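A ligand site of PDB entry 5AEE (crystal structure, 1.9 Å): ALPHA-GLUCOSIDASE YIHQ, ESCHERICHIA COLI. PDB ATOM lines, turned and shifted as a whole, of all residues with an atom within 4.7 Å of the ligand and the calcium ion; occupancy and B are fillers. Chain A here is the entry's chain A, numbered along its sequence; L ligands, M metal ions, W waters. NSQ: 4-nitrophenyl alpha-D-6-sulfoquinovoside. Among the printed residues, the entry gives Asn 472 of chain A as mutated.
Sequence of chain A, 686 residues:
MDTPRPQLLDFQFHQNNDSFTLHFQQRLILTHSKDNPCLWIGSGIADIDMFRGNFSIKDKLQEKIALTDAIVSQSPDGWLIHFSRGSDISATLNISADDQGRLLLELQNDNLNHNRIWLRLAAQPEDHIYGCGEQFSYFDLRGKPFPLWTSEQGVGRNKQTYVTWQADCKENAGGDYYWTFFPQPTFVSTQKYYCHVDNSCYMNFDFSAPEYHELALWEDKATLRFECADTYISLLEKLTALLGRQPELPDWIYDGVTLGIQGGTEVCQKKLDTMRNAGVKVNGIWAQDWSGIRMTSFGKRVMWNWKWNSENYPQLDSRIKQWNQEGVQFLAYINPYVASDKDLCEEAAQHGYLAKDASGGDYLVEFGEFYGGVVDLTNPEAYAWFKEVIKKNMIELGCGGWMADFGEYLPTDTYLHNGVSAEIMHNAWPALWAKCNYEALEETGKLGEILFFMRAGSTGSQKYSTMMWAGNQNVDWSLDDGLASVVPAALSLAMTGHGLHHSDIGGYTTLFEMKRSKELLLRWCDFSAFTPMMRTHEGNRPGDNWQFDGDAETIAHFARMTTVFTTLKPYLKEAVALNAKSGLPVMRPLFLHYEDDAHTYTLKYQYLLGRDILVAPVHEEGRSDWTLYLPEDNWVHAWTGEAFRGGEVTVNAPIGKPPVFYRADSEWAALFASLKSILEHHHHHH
An oxygen (O33) of the ligand lies close to the backbone carbonyl oxygen of Phe 367, at 3.4 Å. O5 of the ligand lies close to OD2 of Asp 405, at 2.9 Å. Merely in contact with the ligand: Arg 52, Glu 152, Phe 298, Tyr 333, Phe 406, Trp 469 and Tyr 508. 18 residues have an atom within 4 Å of the ligand: Arg 52, Glu 152, Gln 288, Phe 298, Arg 301, Val 302, Trp 304, Tyr 333, Phe 367, Met 403, Asp 405, Phe 406, Tyr 409, Arg 455, Trp 469, Asn 472, Tyr 508 and His 537.
OE1 of Gln 153 binds the calcium ion, 2.2 Å away. O of Asn 472 is bound to the calcium ion (2.3 Å). O of Gly 154 binds the calcium ion. Water W5 binds the calcium ion (2.4 Å). Water W4 binds the calcium ion, at 2.4 Å. The side-chain carboxylate (OD1) of Asp 481 is bound to the calcium ion, at 2.4 Å. OD2 of Asp 481 binds the calcium ion, 2.5 Å away. The calcium ion has seven donor atoms within binding distance.
Within 4 Å of the calcium ion: Gln 153, Gly 154, Asn 472 and Asp 481.
Water W4 lies within hydrogen-bond range of OD1 of Asn 474 (2.7 Å) and OG1 of Thr 509 (2.7 Å). Water W1 lies within hydrogen-bond range of O33 of the ligand, O of Phe 367, NH2 of Arg 301 and OH of Tyr 409. Water W2 lies within hydrogen-bond range of the side-chain amide oxygen (OD1) of Asn 472 (2.6 Å), an oxygen (O3) of the ligand (2.7 Å) and the indole nitrogen (NE1) of Trp 469 (2.9 Å). Water W3 lies within hydrogen-bond range of OH of Tyr 508, O11 of the ligand, O of Lys 300 and NE2 of Gln 288.
O of Gln 153 is in hydrogen-bond range of NE of Arg 157, 2.8 Å away. O of Asp 481 sits at hydrogen-bond distance from N of Asn 474, 2.8 Å away. The backbone carbonyl oxygen (O) of Val 302 lies close to the indole nitrogen (NE1) of Trp 304, 3.5 Å away. OD1 of Asp 405 lies within salt-bridge range of NE of Arg 455, at 2.7 Å. The side-chain hydroxyl (OH) of Tyr 333 is in hydrogen-bond range of the side-chain carboxylate (OD2) of Asp 405, 2.6 Å away. The side-chain hydroxyl (OH) of Tyr 409 sits close to the backbone carbonyl oxygen (O) of Arg 52 (3.1 Å). OE1 of Glu 152 is in salt-bridge range of NH1 of Arg 455 (3.3 Å). The backbone NH of Tyr 508 sits at hydrogen-bond distance from the backbone carbonyl oxygen of Gln 473 (2.8 Å).
The side-chain amide oxygen (OD1) of Asn 472 sits at hydrogen-bond distance from an oxygen (O2) of the ligand (2.8 Å). OE1 of Gln 288 lies within hydrogen-bond range of O4 of the ligand, at 2.5 Å. The guanidinium group of Arg 301 lies within salt-bridge range of an oxygen (O12) of the ligand (2.8 Å). N of Val 302 sits at hydrogen-bond distance from O13 of the ligand (2.8 Å). NE2 of His 537 lies within hydrogen-bond range of O3 of the ligand (2.8 Å). An oxygen (O34) of the ligand lies within hydrogen-bond range of the side-chain hydroxyl (OH) of Tyr 409 (3.0 Å). NE1 of Trp 304 is in hydrogen-bond range of O13 of the ligand (3.0 Å). The guanidinium group (NE) of Arg 455 is in hydrogen-bond range of an oxygen (O2) of the ligand (3.3 Å). The side-chain sulfur (SD) of Met 403 lies close to an oxygen (O3) of the ligand, 3.6 Å away.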
ATOM      1  N   ARG A  52     -27.928 -13.859   9.134  1.00  0.00           N
ATOM      2  CA  ARG A  52     -26.815 -12.956   8.852  1.00  0.00           C
ATOM      3  C   ARG A  52     -26.013 -13.331   7.622  1.00  0.00           C
ATOM      4  O   ARG A  52     -24.778 -13.357   7.641  1.00  0.00           O
ATOM      5  CB  ARG A  52     -25.952 -12.838  10.087  1.00  0.00           C
ATOM      6  CG  ARG A  52     -26.680 -12.126  11.201  1.00  0.00           C
ATOM      7  CD  ARG A  52     -25.795 -11.974  12.417  1.00  0.00           C
ATOM      8  NE  ARG A  52     -26.577 -11.519  13.540  1.00  0.00           N
ATOM      9  CZ  ARG A  52     -26.164 -11.465  14.789  1.00  0.00           C
ATOM     10  NH1 ARG A  52     -24.942 -11.855  15.108  1.00  0.00           N
ATOM     11  NH2 ARG A  52     -26.972 -10.998  15.731  1.00  0.00           N
ATOM     12  N   GLU A 152     -22.661 -15.350   2.453  1.00  0.00           N
ATOM     13  CA  GLU A 152     -21.370 -15.129   3.137  1.00  0.00           C
ATOM     14  C   GLU A 152     -20.409 -16.248   2.853  1.00  0.00           C
ATOM     15  O   GLU A 152     -20.748 -17.411   2.678  1.00  0.00           O
ATOM     16  CB  GLU A 152     -21.470 -14.961   4.648  1.00  0.00           C
ATOM     17  CG  GLU A 152     -22.443 -13.906   5.133  1.00  0.00           C
ATOM     18  CD  GLU A 152     -22.267 -12.550   4.430  1.00  0.00           C
ATOM     19  OE1 GLU A 152     -21.168 -11.966   4.532  1.00  0.00           O
ATOM     20  OE2 GLU A 152     -23.247 -12.121   3.730  1.00  0.00           O
ATOM     21  N   GLN A 153     -19.175 -15.856   2.744  1.00  0.00           N
ATOM     22  CA  GLN A 153     -18.098 -16.728   2.280  1.00  0.00           C
ATOM     23  C   GLN A 153     -17.609 -17.780   3.328  1.00  0.00           C
ATOM     24  O   GLN A 153     -16.918 -18.719   2.969  1.00  0.00           O
ATOM     25  CB  GLN A 153     -16.994 -15.821   1.843  1.00  0.00           C
ATOM     26  CG  GLN A 153     -15.892 -16.461   1.095  1.00  0.00           C
ATOM     27  CD  GLN A 153     -14.614 -16.392   1.837  1.00  0.00           C
ATOM     28  OE1 GLN A 153     -14.539 -16.118   3.060  1.00  0.00           O
ATOM     29  NE2 GLN A 153     -13.575 -16.718   1.126  1.00  0.00           N
ATOM     30  N   GLY A 154     -17.974 -17.617   4.599  1.00  0.00           N
ATOM     31  CA  GLY A 154     -17.448 -18.493   5.631  1.00  0.00           C
ATOM     32  C   GLY A 154     -16.312 -17.862   6.414  1.00  0.00           C
ATOM     33  O   GLY A 154     -15.461 -17.186   5.857  1.00  0.00           O
ATOM     34  N   VAL A 155     -16.273 -18.178   7.693  1.00  0.00           N
ATOM     35  CA  VAL A 155     -15.167 -17.854   8.570  1.00  0.00           C
ATOM     36  C   VAL A 155     -14.434 -19.140   8.929  1.00  0.00           C
ATOM     37  O   VAL A 155     -14.907 -19.857   9.795  1.00  0.00           O
ATOM     38  CB  VAL A 155     -15.645 -17.156   9.861  1.00  0.00           C
ATOM     39  CG1 VAL A 155     -14.499 -16.987  10.820  1.00  0.00           C
ATOM     40  CG2 VAL A 155     -16.317 -15.825   9.517  1.00  0.00           C
ATOM     41  N   ARG A 157     -14.044 -21.876   6.926  1.00  0.00           N
ATOM     42  CA  ARG A 157     -14.451 -22.543   5.642  1.00  0.00           C
ATOM     43  C   ARG A 157     -14.038 -24.001   5.590  1.00  0.00           C
ATOM     44  O   ARG A 157     -14.126 -24.593   4.525  1.00  0.00           O
ATOM     45  CB  ARG A 157     -13.883 -21.846   4.408  1.00  0.00           C
ATOM     46  CG  ARG A 157     -14.216 -20.332   4.496  1.00  0.00           C
ATOM     47  CD  ARG A 157     -13.775 -19.545   3.313  1.00  0.00           C
ATOM     48  NE  ARG A 157     -14.566 -20.012   2.138  1.00  0.00           N
ATOM     49  CZ  ARG A 157     -14.178 -20.900   1.251  1.00  0.00           C
ATOM     50  NH1 ARG A 157     -12.953 -21.392   1.299  1.00  0.00           N
ATOM     51  NH2 ARG A 157     -15.004 -21.277   0.257  1.00  0.00           N
ATOM     52  N   TRP A 286      -8.973   5.173   1.767  1.00  0.00           N
ATOM     53  CA  TRP A 286     -10.243   4.524   1.735  1.00  0.00           C
ATOM     54  C   TRP A 286     -10.772   4.495   3.167  1.00  0.00           C
ATOM     55  O   TRP A 286     -10.164   3.830   4.073  1.00  0.00           O
ATOM     56  CB  TRP A 286     -10.129   3.095   1.204  1.00  0.00           C
ATOM     57  CG  TRP A 286     -11.332   2.390   1.425  1.00  0.00           C
ATOM     58  CD1 TRP A 286     -12.570   2.689   0.927  1.00  0.00           C
ATOM     59  CD2 TRP A 286     -11.482   1.145   2.138  1.00  0.00           C
ATOM     60  NE1 TRP A 286     -13.497   1.779   1.382  1.00  0.00           N
ATOM     61  CE2 TRP A 286     -12.860   0.824   2.125  1.00  0.00           C
ATOM     62  CE3 TRP A 286     -10.601   0.323   2.853  1.00  0.00           C
ATOM     63  CZ2 TRP A 286     -13.374  -0.308   2.764  1.00  0.00           C
ATOM     64  CZ3 TRP A 286     -11.108  -0.799   3.498  1.00  0.00           C
ATOM     65  CH2 TRP A 286     -12.505  -1.093   3.448  1.00  0.00           C
ATOM     66  N   GLN A 288     -13.987   3.677   5.129  1.00  0.00           N
ATOM     67  CA  GLN A 288     -15.267   3.092   4.987  1.00  0.00           C
ATOM     68  C   GLN A 288     -16.276   3.752   5.978  1.00  0.00           C
ATOM     69  O   GLN A 288     -17.449   3.749   5.739  1.00  0.00           O
ATOM     70  CB  GLN A 288     -15.235   1.533   5.251  1.00  0.00           C
ATOM     71  CG  GLN A 288     -14.759   1.150   6.635  1.00  0.00           C
ATOM     72  CD  GLN A 288     -15.041  -0.333   6.839  1.00  0.00           C
ATOM     73  OE1 GLN A 288     -15.295  -1.088   5.871  1.00  0.00           O
ATOM     74  NE2 GLN A 288     -15.048  -0.759   8.098  1.00  0.00           N
ATOM     75  N   PHE A 298     -19.357  -7.693  16.908  1.00  0.00           N
ATOM     76  CA  PHE A 298     -18.462  -8.091  15.797  1.00  0.00           C
ATOM     77  C   PHE A 298     -17.277  -7.176  15.698  1.00  0.00           C
ATOM     78  O   PHE A 298     -16.144  -7.599  15.485  1.00  0.00           O
ATOM     79  CB  PHE A 298     -19.249  -8.100  14.485  1.00  0.00           C
ATOM     80  CG  PHE A 298     -18.446  -8.530  13.295  1.00  0.00           C
ATOM     81  CD1 PHE A 298     -18.265  -9.868  13.032  1.00  0.00           C
ATOM     82  CD2 PHE A 298     -17.933  -7.601  12.384  1.00  0.00           C
ATOM     83  CE1 PHE A 298     -17.576 -10.286  11.925  1.00  0.00           C
ATOM     84  CE2 PHE A 298     -17.223  -8.033  11.276  1.00  0.00           C
ATOM     85  CZ  PHE A 298     -17.028  -9.364  11.065  1.00  0.00           C
ATOM     86  N   LYS A 300     -16.006  -2.823  14.801  1.00  0.00           N
ATOM     87  CA  LYS A 300     -16.290  -1.478  14.341  1.00  0.00           C
ATOM     88  C   LYS A 300     -16.828  -1.630  12.905  1.00  0.00           C
ATOM     89  O   LYS A 300     -16.139  -2.133  12.005  1.00  0.00           O
ATOM     90  CB  LYS A 300     -15.047  -0.674  14.470  1.00  0.00           C
ATOM     91  CG  LYS A 300     -15.090   0.759  14.012  1.00  0.00           C
ATOM     92  CD  LYS A 300     -13.907   1.522  14.650  1.00  0.00           C
ATOM     93  CE  LYS A 300     -13.464   2.772  13.868  1.00  0.00           C
ATOM     94  NZ  LYS A 300     -12.207   3.401  14.399  1.00  0.00           N
ATOM     95  N   ARG A 301     -18.108  -1.320  12.711  1.00  0.00           N
ATOM     96  CA  ARG A 301     -18.779  -1.416  11.419  1.00  0.00           C
ATOM     97  C   ARG A 301     -19.134  -0.034  10.934  1.00  0.00           C
ATOM     98  O   ARG A 301     -18.919   0.975  11.626  1.00  0.00           O
ATOM     99  CB  ARG A 301     -19.970  -2.340  11.461  1.00  0.00           C
ATOM    100  CG  ARG A 301     -19.530  -3.722  11.907  1.00  0.00           C
ATOM    101  CD  ARG A 301     -20.638  -4.721  11.830  1.00  0.00           C
ATOM    102  NE  ARG A 301     -20.995  -5.048  10.483  1.00  0.00           N
ATOM    103  CZ  ARG A 301     -22.037  -5.798  10.139  1.00  0.00           C
ATOM    104  NH1 ARG A 301     -22.864  -6.358  11.069  1.00  0.00           N
ATOM    105  NH2 ARG A 301     -22.245  -6.003   8.847  1.00  0.00           N
ATOM    106  N   VAL A 302     -19.675   0.053   9.733  1.00  0.00           N
ATOM    107  CA  VAL A 302     -19.977   1.344   9.128  1.00  0.00           C
ATOM    108  C   VAL A 302     -21.409   1.629   9.523  1.00  0.00           C
ATOM    109  O   VAL A 302     -22.193   0.679   9.700  1.00  0.00           O
ATOM    110  CB  VAL A 302     -19.824   1.262   7.622  1.00  0.00           C
ATOM    111  CG1 VAL A 302     -20.236   2.566   6.948  1.00  0.00           C
ATOM    112  CG2 VAL A 302     -18.374   0.940   7.266  1.00  0.00           C
ATOM    113  N   TRP A 304     -24.718   2.375   8.210  1.00  0.00           N
ATOM    114  CA  TRP A 304     -25.304   2.211   6.835  1.00  0.00           C
ATOM    115  C   TRP A 304     -26.361   3.201   6.389  1.00  0.00           C
ATOM    116  O   TRP A 304     -27.522   2.886   6.027  1.00  0.00           O
ATOM    117  CB  TRP A 304     -25.788   0.781   6.599  1.00  0.00           C
ATOM    118  CG  TRP A 304     -24.816  -0.298   6.716  1.00  0.00           C
ATOM    119  CD1 TRP A 304     -23.482  -0.237   7.067  1.00  0.00           C
ATOM    120  CD2 TRP A 304     -25.100  -1.665   6.539  1.00  0.00           C
ATOM    121  NE1 TRP A 304     -22.937  -1.490   7.065  1.00  0.00           N
ATOM    122  CE2 TRP A 304     -23.891  -2.383   6.740  1.00  0.00           C
ATOM    123  CE3 TRP A 304     -26.226  -2.354   6.178  1.00  0.00           C
ATOM    124  CZ2 TRP A 304     -23.815  -3.745   6.657  1.00  0.00           C
ATOM    125  CZ3 TRP A 304     -26.140  -3.734   6.063  1.00  0.00           C
ATOM    126  CH2 TRP A 304     -24.941  -4.397   6.280  1.00  0.00           C
ATOM    127  N   TYR A 333     -17.624   3.953   0.974  1.00  0.00           N
ATOM    128  CA  TYR A 333     -18.230   2.637   1.207  1.00  0.00           C
ATOM    129  C   TYR A 333     -19.754   2.814   0.992  1.00  0.00           C
ATOM    130  O   TYR A 333     -20.386   3.780   1.492  1.00  0.00           O
ATOM    131  CB  TYR A 333     -17.945   2.155   2.628  1.00  0.00           C
ATOM    132  CG  TYR A 333     -18.624   0.811   2.930  1.00  0.00           C
ATOM    133  CD1 TYR A 333     -19.972   0.765   3.324  1.00  0.00           C
ATOM    134  CD2 TYR A 333     -17.987  -0.359   2.777  1.00  0.00           C
ATOM    135  CE1 TYR A 333     -20.601  -0.445   3.554  1.00  0.00           C
ATOM    136  CE2 TYR A 333     -18.640  -1.623   3.030  1.00  0.00           C
ATOM    137  CZ  TYR A 333     -19.946  -1.623   3.377  1.00  0.00           C
ATOM    138  OH  TYR A 333     -20.648  -2.784   3.645  1.00  0.00           O
ATOM    139  N   PHE A 367     -28.839  -7.554  10.343  1.00  0.00           N
ATOM    140  CA  PHE A 367     -27.484  -7.508   9.731  1.00  0.00           C
ATOM    141  C   PHE A 367     -26.351  -7.675  10.749  1.00  0.00           C
ATOM    142  O   PHE A 367     -25.157  -7.612  10.380  1.00  0.00           O
ATOM    143  CB  PHE A 367     -27.316  -6.159   8.984  1.00  0.00           C
ATOM    144  CG  PHE A 367     -27.984  -6.107   7.655  1.00  0.00           C
ATOM    145  CD1 PHE A 367     -27.519  -6.895   6.592  1.00  0.00           C
ATOM    146  CD2 PHE A 367     -29.097  -5.311   7.452  1.00  0.00           C
ATOM    147  CE1 PHE A 367     -28.177  -6.907   5.372  1.00  0.00           C
ATOM    148  CE2 PHE A 367     -29.743  -5.296   6.221  1.00  0.00           C
ATOM    149  CZ  PHE A 367     -29.277  -6.087   5.195  1.00  0.00           C
ATOM    150  N   MET A 403     -15.690   1.015  -2.001  1.00  0.00           N
ATOM    151  CA  MET A 403     -16.220  -0.356  -1.782  1.00  0.00           C
ATOM    152  C   MET A 403     -17.731  -0.361  -2.031  1.00  0.00           C
ATOM    153  O   MET A 403     -18.478   0.325  -1.300  1.00  0.00           O
ATOM    154  CB  MET A 403     -15.891  -0.823  -0.358  1.00  0.00           C
ATOM    155  CG  MET A 403     -16.354  -2.267  -0.034  1.00  0.00           C
ATOM    156  SD  MET A 403     -15.732  -2.779   1.550  1.00  0.00           S
ATOM    157  CE  MET A 403     -14.090  -3.237   1.111  1.00  0.00           C
ATOM    158  N   ASP A 405     -20.368  -2.902  -1.609  1.00  0.00           N
ATOM    159  CA  ASP A 405     -20.283  -4.127  -0.823  1.00  0.00           C
ATOM    160  C   ASP A 405     -21.619  -4.810  -0.866  1.00  0.00           C
ATOM    161  O   ASP A 405     -22.578  -4.251  -1.342  1.00  0.00           O
ATOM    162  CB  ASP A 405     -19.815  -3.779   0.564  1.00  0.00           C
ATOM    163  CG  ASP A 405     -19.465  -4.979   1.426  1.00  0.00           C
ATOM    164  OD1 ASP A 405     -19.219  -6.103   0.925  1.00  0.00           O
ATOM    165  OD2 ASP A 405     -19.350  -4.754   2.635  1.00  0.00           O
ATOM    166  N   PHE A 406     -21.645  -6.050  -0.420  1.00  0.00           N
ATOM    167  CA  PHE A 406     -22.828  -6.854  -0.220  1.00  0.00           C
ATOM    168  C   PHE A 406     -23.489  -7.101  -1.545  1.00  0.00           C
ATOM    169  O   PHE A 406     -22.844  -6.933  -2.574  1.00  0.00           O
ATOM    170  CB  PHE A 406     -23.804  -6.325   0.868  1.00  0.00           C
ATOM    171  CG  PHE A 406     -23.272  -6.431   2.240  1.00  0.00           C
ATOM    172  CD1 PHE A 406     -22.505  -5.431   2.771  1.00  0.00           C
ATOM    173  CD2 PHE A 406     -23.570  -7.560   3.017  1.00  0.00           C
ATOM    174  CE1 PHE A 406     -21.971  -5.584   4.058  1.00  0.00           C
ATOM    175  CE2 PHE A 406     -23.099  -7.681   4.311  1.00  0.00           C
ATOM    176  CZ  PHE A 406     -22.250  -6.722   4.797  1.00  0.00           C
ATOM    177  N   TYR A 409     -27.129 -11.058   0.261  1.00  0.00           N
ATOM    178  CA  TYR A 409     -27.913 -11.222   1.480  1.00  0.00           C
ATOM    179  C   TYR A 409     -29.381 -11.214   1.286  1.00  0.00           C
ATOM    180  O   TYR A 409     -30.094 -11.141   2.285  1.00  0.00           O
ATOM    181  CB  TYR A 409     -27.658 -10.033   2.403  1.00  0.00           C
ATOM    182  CG  TYR A 409     -27.185 -10.242   3.839  1.00  0.00           C
ATOM    183  CD1 TYR A 409     -25.834 -10.331   4.114  1.00  0.00           C
ATOM    184  CD2 TYR A 409     -28.085 -10.166   4.927  1.00  0.00           C
ATOM    185  CE1 TYR A 409     -25.355 -10.407   5.436  1.00  0.00           C
ATOM    186  CE2 TYR A 409     -27.622 -10.238   6.261  1.00  0.00           C
ATOM    187  CZ  TYR A 409     -26.242 -10.368   6.504  1.00  0.00           C
ATOM    188  OH  TYR A 409     -25.671 -10.430   7.807  1.00  0.00           O
ATOM    189  N   ARG A 455     -17.538  -7.271  -3.874  1.00  0.00           N
ATOM    190  CA  ARG A 455     -17.274  -8.589  -3.225  1.00  0.00           C
ATOM    191  C   ARG A 455     -18.233  -9.578  -3.852  1.00  0.00           C
ATOM    192  O   ARG A 455     -17.793 -10.491  -4.551  1.00  0.00           O
ATOM    193  CB  ARG A 455     -17.498  -8.401  -1.700  1.00  0.00           C
ATOM    194  CG  ARG A 455     -17.457  -9.657  -0.841  1.00  0.00           C
ATOM    195  CD  ARG A 455     -17.333  -9.355   0.631  1.00  0.00           C
ATOM    196  NE  ARG A 455     -18.550  -8.745   1.179  1.00  0.00           N
ATOM    197  CZ  ARG A 455     -19.550  -9.362   1.768  1.00  0.00           C
ATOM    198  NH1 ARG A 455     -19.563 -10.687   1.985  1.00  0.00           N
ATOM    199  NH2 ARG A 455     -20.572  -8.630   2.188  1.00  0.00           N
ATOM    200  N   TRP A 469     -12.902  -7.526  -5.206  1.00  0.00           N
ATOM    201  CA  TRP A 469     -11.967  -7.831  -4.144  1.00  0.00           C
ATOM    202  C   TRP A 469     -12.386  -9.166  -3.524  1.00  0.00           C
ATOM    203  O   TRP A 469     -13.541  -9.534  -3.612  1.00  0.00           O
ATOM    204  CB  TRP A 469     -11.719  -6.720  -3.148  1.00  0.00           C
ATOM    205  CG  TRP A 469     -12.475  -6.754  -1.871  1.00  0.00           C
ATOM    206  CD1 TRP A 469     -12.014  -7.283  -0.678  1.00  0.00           C
ATOM    207  CD2 TRP A 469     -13.750  -6.262  -1.620  1.00  0.00           C
ATOM    208  NE1 TRP A 469     -12.956  -7.156   0.263  1.00  0.00           N
ATOM    209  CE2 TRP A 469     -14.043  -6.525  -0.260  1.00  0.00           C
ATOM    210  CE3 TRP A 469     -14.733  -5.625  -2.421  1.00  0.00           C
ATOM    211  CZ2 TRP A 469     -15.225  -6.191   0.321  1.00  0.00           C
ATOM    212  CZ3 TRP A 469     -15.915  -5.245  -1.806  1.00  0.00           C
ATOM    213  CH2 TRP A 469     -16.168  -5.557  -0.459  1.00  0.00           C
ATOM    214  N   ASN A 472     -13.722 -11.301   2.704  1.00  0.00           N
ATOM    215  CA  ASN A 472     -13.140 -11.376   4.062  1.00  0.00           C
ATOM    216  C   ASN A 472     -12.373 -12.632   4.281  1.00  0.00           C
ATOM    217  O   ASN A 472     -12.996 -13.701   4.447  1.00  0.00           O
ATOM    218  CB  ASN A 472     -14.291 -11.289   5.062  1.00  0.00           C
ATOM    219  CG  ASN A 472     -14.981  -9.961   5.079  1.00  0.00           C
ATOM    220  OD1 ASN A 472     -14.521  -8.988   4.480  1.00  0.00           O
ATOM    221  ND2 ASN A 472     -16.095  -9.914   5.779  1.00  0.00           N
ATOM    222  N   GLN A 473     -11.068 -12.512   4.201  1.00  0.00           N
ATOM    223  CA  GLN A 473     -10.144 -13.489   4.720  1.00  0.00           C
ATOM    224  C   GLN A 473      -9.993 -13.290   6.216  1.00  0.00           C
ATOM    225  O   GLN A 473      -9.939 -12.214   6.748  1.00  0.00           O
ATOM    226  CB  GLN A 473      -8.739 -13.390   4.105  1.00  0.00           C
ATOM    227  CG  GLN A 473      -8.683 -13.962   2.706  1.00  0.00           C
ATOM    228  CD  GLN A 473      -9.424 -13.139   1.713  1.00  0.00           C
ATOM    229  OE1 GLN A 473      -9.068 -11.966   1.451  1.00  0.00           O
ATOM    230  NE2 GLN A 473     -10.469 -13.722   1.159  1.00  0.00           N
ATOM    231  N   ASN A 474      -9.812 -14.417   6.887  1.00  0.00           N
ATOM    232  CA  ASN A 474      -9.306 -14.398   8.244  1.00  0.00           C
ATOM    233  C   ASN A 474      -7.968 -13.792   8.266  1.00  0.00           C
ATOM    234  O   ASN A 474      -7.193 -13.947   7.315  1.00  0.00           O
ATOM    235  CB  ASN A 474      -9.194 -15.856   8.790  1.00  0.00           C
ATOM    236  CG  ASN A 474     -10.537 -16.495   9.036  1.00  0.00           C
ATOM    237  OD1 ASN A 474     -11.531 -15.819   9.115  1.00  0.00           O
ATOM    238  ND2 ASN A 474     -10.556 -17.825   9.334  1.00  0.00           N
ATOM    239  N   ASP A 481      -9.073 -20.021   4.257  1.00  0.00           N
ATOM    240  CA  ASP A 481      -9.563 -18.666   4.524  1.00  0.00           C
ATOM    241  C   ASP A 481      -8.520 -17.594   4.832  1.00  0.00           C
ATOM    242  O   ASP A 481      -8.882 -16.529   5.249  1.00  0.00           O
ATOM    243  CB  ASP A 481     -10.636 -18.721   5.600  1.00  0.00           C
ATOM    244  CG  ASP A 481     -11.715 -17.610   5.461  1.00  0.00           C
ATOM    245  OD1 ASP A 481     -11.789 -16.861   4.439  1.00  0.00           O
ATOM    246  OD2 ASP A 481     -12.535 -17.444   6.433  1.00  0.00           O
ATOM    247  N   TYR A 508      -9.071  -9.562   6.847  1.00  0.00           N
ATOM    248  CA  TYR A 508     -10.112  -8.784   7.503  1.00  0.00           C
ATOM    249  C   TYR A 508     -10.613  -9.318   8.838  1.00  0.00           C
ATOM    250  O   TYR A 508     -10.583  -8.598   9.824  1.00  0.00           O
ATOM    251  CB  TYR A 508     -11.322  -8.584   6.541  1.00  0.00           C
ATOM    252  CG  TYR A 508     -12.498  -7.910   7.191  1.00  0.00           C
ATOM    253  CD1 TYR A 508     -12.554  -6.549   7.285  1.00  0.00           C
ATOM    254  CD2 TYR A 508     -13.551  -8.656   7.704  1.00  0.00           C
ATOM    255  CE1 TYR A 508     -13.658  -5.930   7.862  1.00  0.00           C
ATOM    256  CE2 TYR A 508     -14.663  -8.051   8.312  1.00  0.00           C
ATOM    257  CZ  TYR A 508     -14.731  -6.665   8.363  1.00  0.00           C
ATOM    258  OH  TYR A 508     -15.805  -6.009   9.002  1.00  0.00           O
ATOM    259  N   THR A 509     -11.006 -10.604   8.848  1.00  0.00           N
ATOM    260  CA  THR A 509     -11.777 -11.174   9.875  1.00  0.00           C
ATOM    261  C   THR A 509     -10.960 -11.479  11.123  1.00  0.00           C
ATOM    262  O   THR A 509     -10.025 -12.258  11.108  1.00  0.00           O
ATOM    263  CB  THR A 509     -12.464 -12.465   9.392  1.00  0.00           C
ATOM    264  OG1 THR A 509     -13.170 -12.186   8.150  1.00  0.00           O
ATOM    265  CG2 THR A 509     -13.448 -13.001  10.550  1.00  0.00           C
ATOM    266  N   HIS A 537      -6.779  -2.765   4.752  1.00  0.00           N
ATOM    267  CA  HIS A 537      -7.989  -2.779   5.604  1.00  0.00           C
ATOM    268  C   HIS A 537      -7.537  -2.850   7.045  1.00  0.00           C
ATOM    269  O   HIS A 537      -6.667  -3.650   7.367  1.00  0.00           O
ATOM    270  CB  HIS A 537      -8.827  -4.032   5.318  1.00  0.00           C
ATOM    271  CG  HIS A 537     -10.284  -3.871   5.516  1.00  0.00           C
ATOM    272  ND1 HIS A 537     -10.820  -3.235   6.593  1.00  0.00           N
ATOM    273  CD2 HIS A 537     -11.344  -4.317   4.801  1.00  0.00           C
ATOM    274  CE1 HIS A 537     -12.124  -3.274   6.554  1.00  0.00           C
ATOM    275  NE2 HIS A 537     -12.476  -3.912   5.476  1.00  0.00           N
HETATM  276  O12 NSQ L   1     -20.545  -4.411   7.306  1.00  0.00           O
HETATM  277  S10 NSQ L   1     -19.553  -3.371   7.679  1.00  0.00           S
HETATM  278  O13 NSQ L   1     -20.043  -1.970   7.805  1.00  0.00           O
HETATM  279  O11 NSQ L   1     -18.845  -3.846   8.860  1.00  0.00           O
HETATM  280  C6  NSQ L   1     -18.396  -3.228   6.422  1.00  0.00           C
HETATM  281  C5  NSQ L   1     -17.596  -4.486   6.092  1.00  0.00           C
HETATM  282  O5  NSQ L   1     -18.537  -5.316   5.341  1.00  0.00           O
HETATM  283  C1  NSQ L   1     -18.027  -6.450   4.720  1.00  0.00           C
HETATM  284  C2  NSQ L   1     -16.784  -6.115   3.858  1.00  0.00           C
HETATM  285  O2  NSQ L   1     -16.379  -7.312   3.256  1.00  0.00           O
HETATM  286  C3  NSQ L   1     -15.751  -5.442   4.727  1.00  0.00           C
HETATM  287  O3  NSQ L   1     -14.572  -5.118   4.027  1.00  0.00           O
HETATM  288  C4  NSQ L   1     -16.294  -4.170   5.338  1.00  0.00           C
HETATM  289  O4  NSQ L   1     -15.286  -3.612   6.234  1.00  0.00           O
HETATM  290  O1  NSQ L   1     -17.693  -7.323   5.783  1.00  0.00           O
HETATM  291  C25 NSQ L   1     -18.713  -7.942   6.398  1.00  0.00           C
HETATM  292  C26 NSQ L   1     -19.542  -8.797   5.654  1.00  0.00           C
HETATM  293  C27 NSQ L   1     -20.616  -9.365   6.281  1.00  0.00           C
HETATM  294  C28 NSQ L   1     -20.809  -9.149   7.644  1.00  0.00           C
HETATM  295  N32 NSQ L   1     -21.955  -9.713   8.238  1.00  0.00           N
HETATM  296  O33 NSQ L   1     -22.369  -9.235   9.335  1.00  0.00           O
HETATM  297  O34 NSQ L   1     -22.675 -10.547   7.585  1.00  0.00           O
HETATM  298  C29 NSQ L   1     -19.979  -8.281   8.350  1.00  0.00           C
HETATM  299  C30 NSQ L   1     -18.907  -7.671   7.722  1.00  0.00           C
HETATM  300 CA    CA M   1     -13.812 -15.711   5.149  1.00  0.00          CA
HETATM  301  O   HOH W   1     -24.103  -7.803   7.887  1.00  0.00           O
HETATM  302  O   HOH W   2     -13.110  -7.225   3.191  1.00  0.00           O
HETATM  303  O   HOH W   3     -16.064  -3.559   9.268  1.00  0.00           O
HETATM  304  O   HOH W   4     -13.075 -14.751   7.178  1.00  0.00           O
HETATM  305  O   HOH W   5     -15.801 -14.472   5.365  1.00  0.00           O
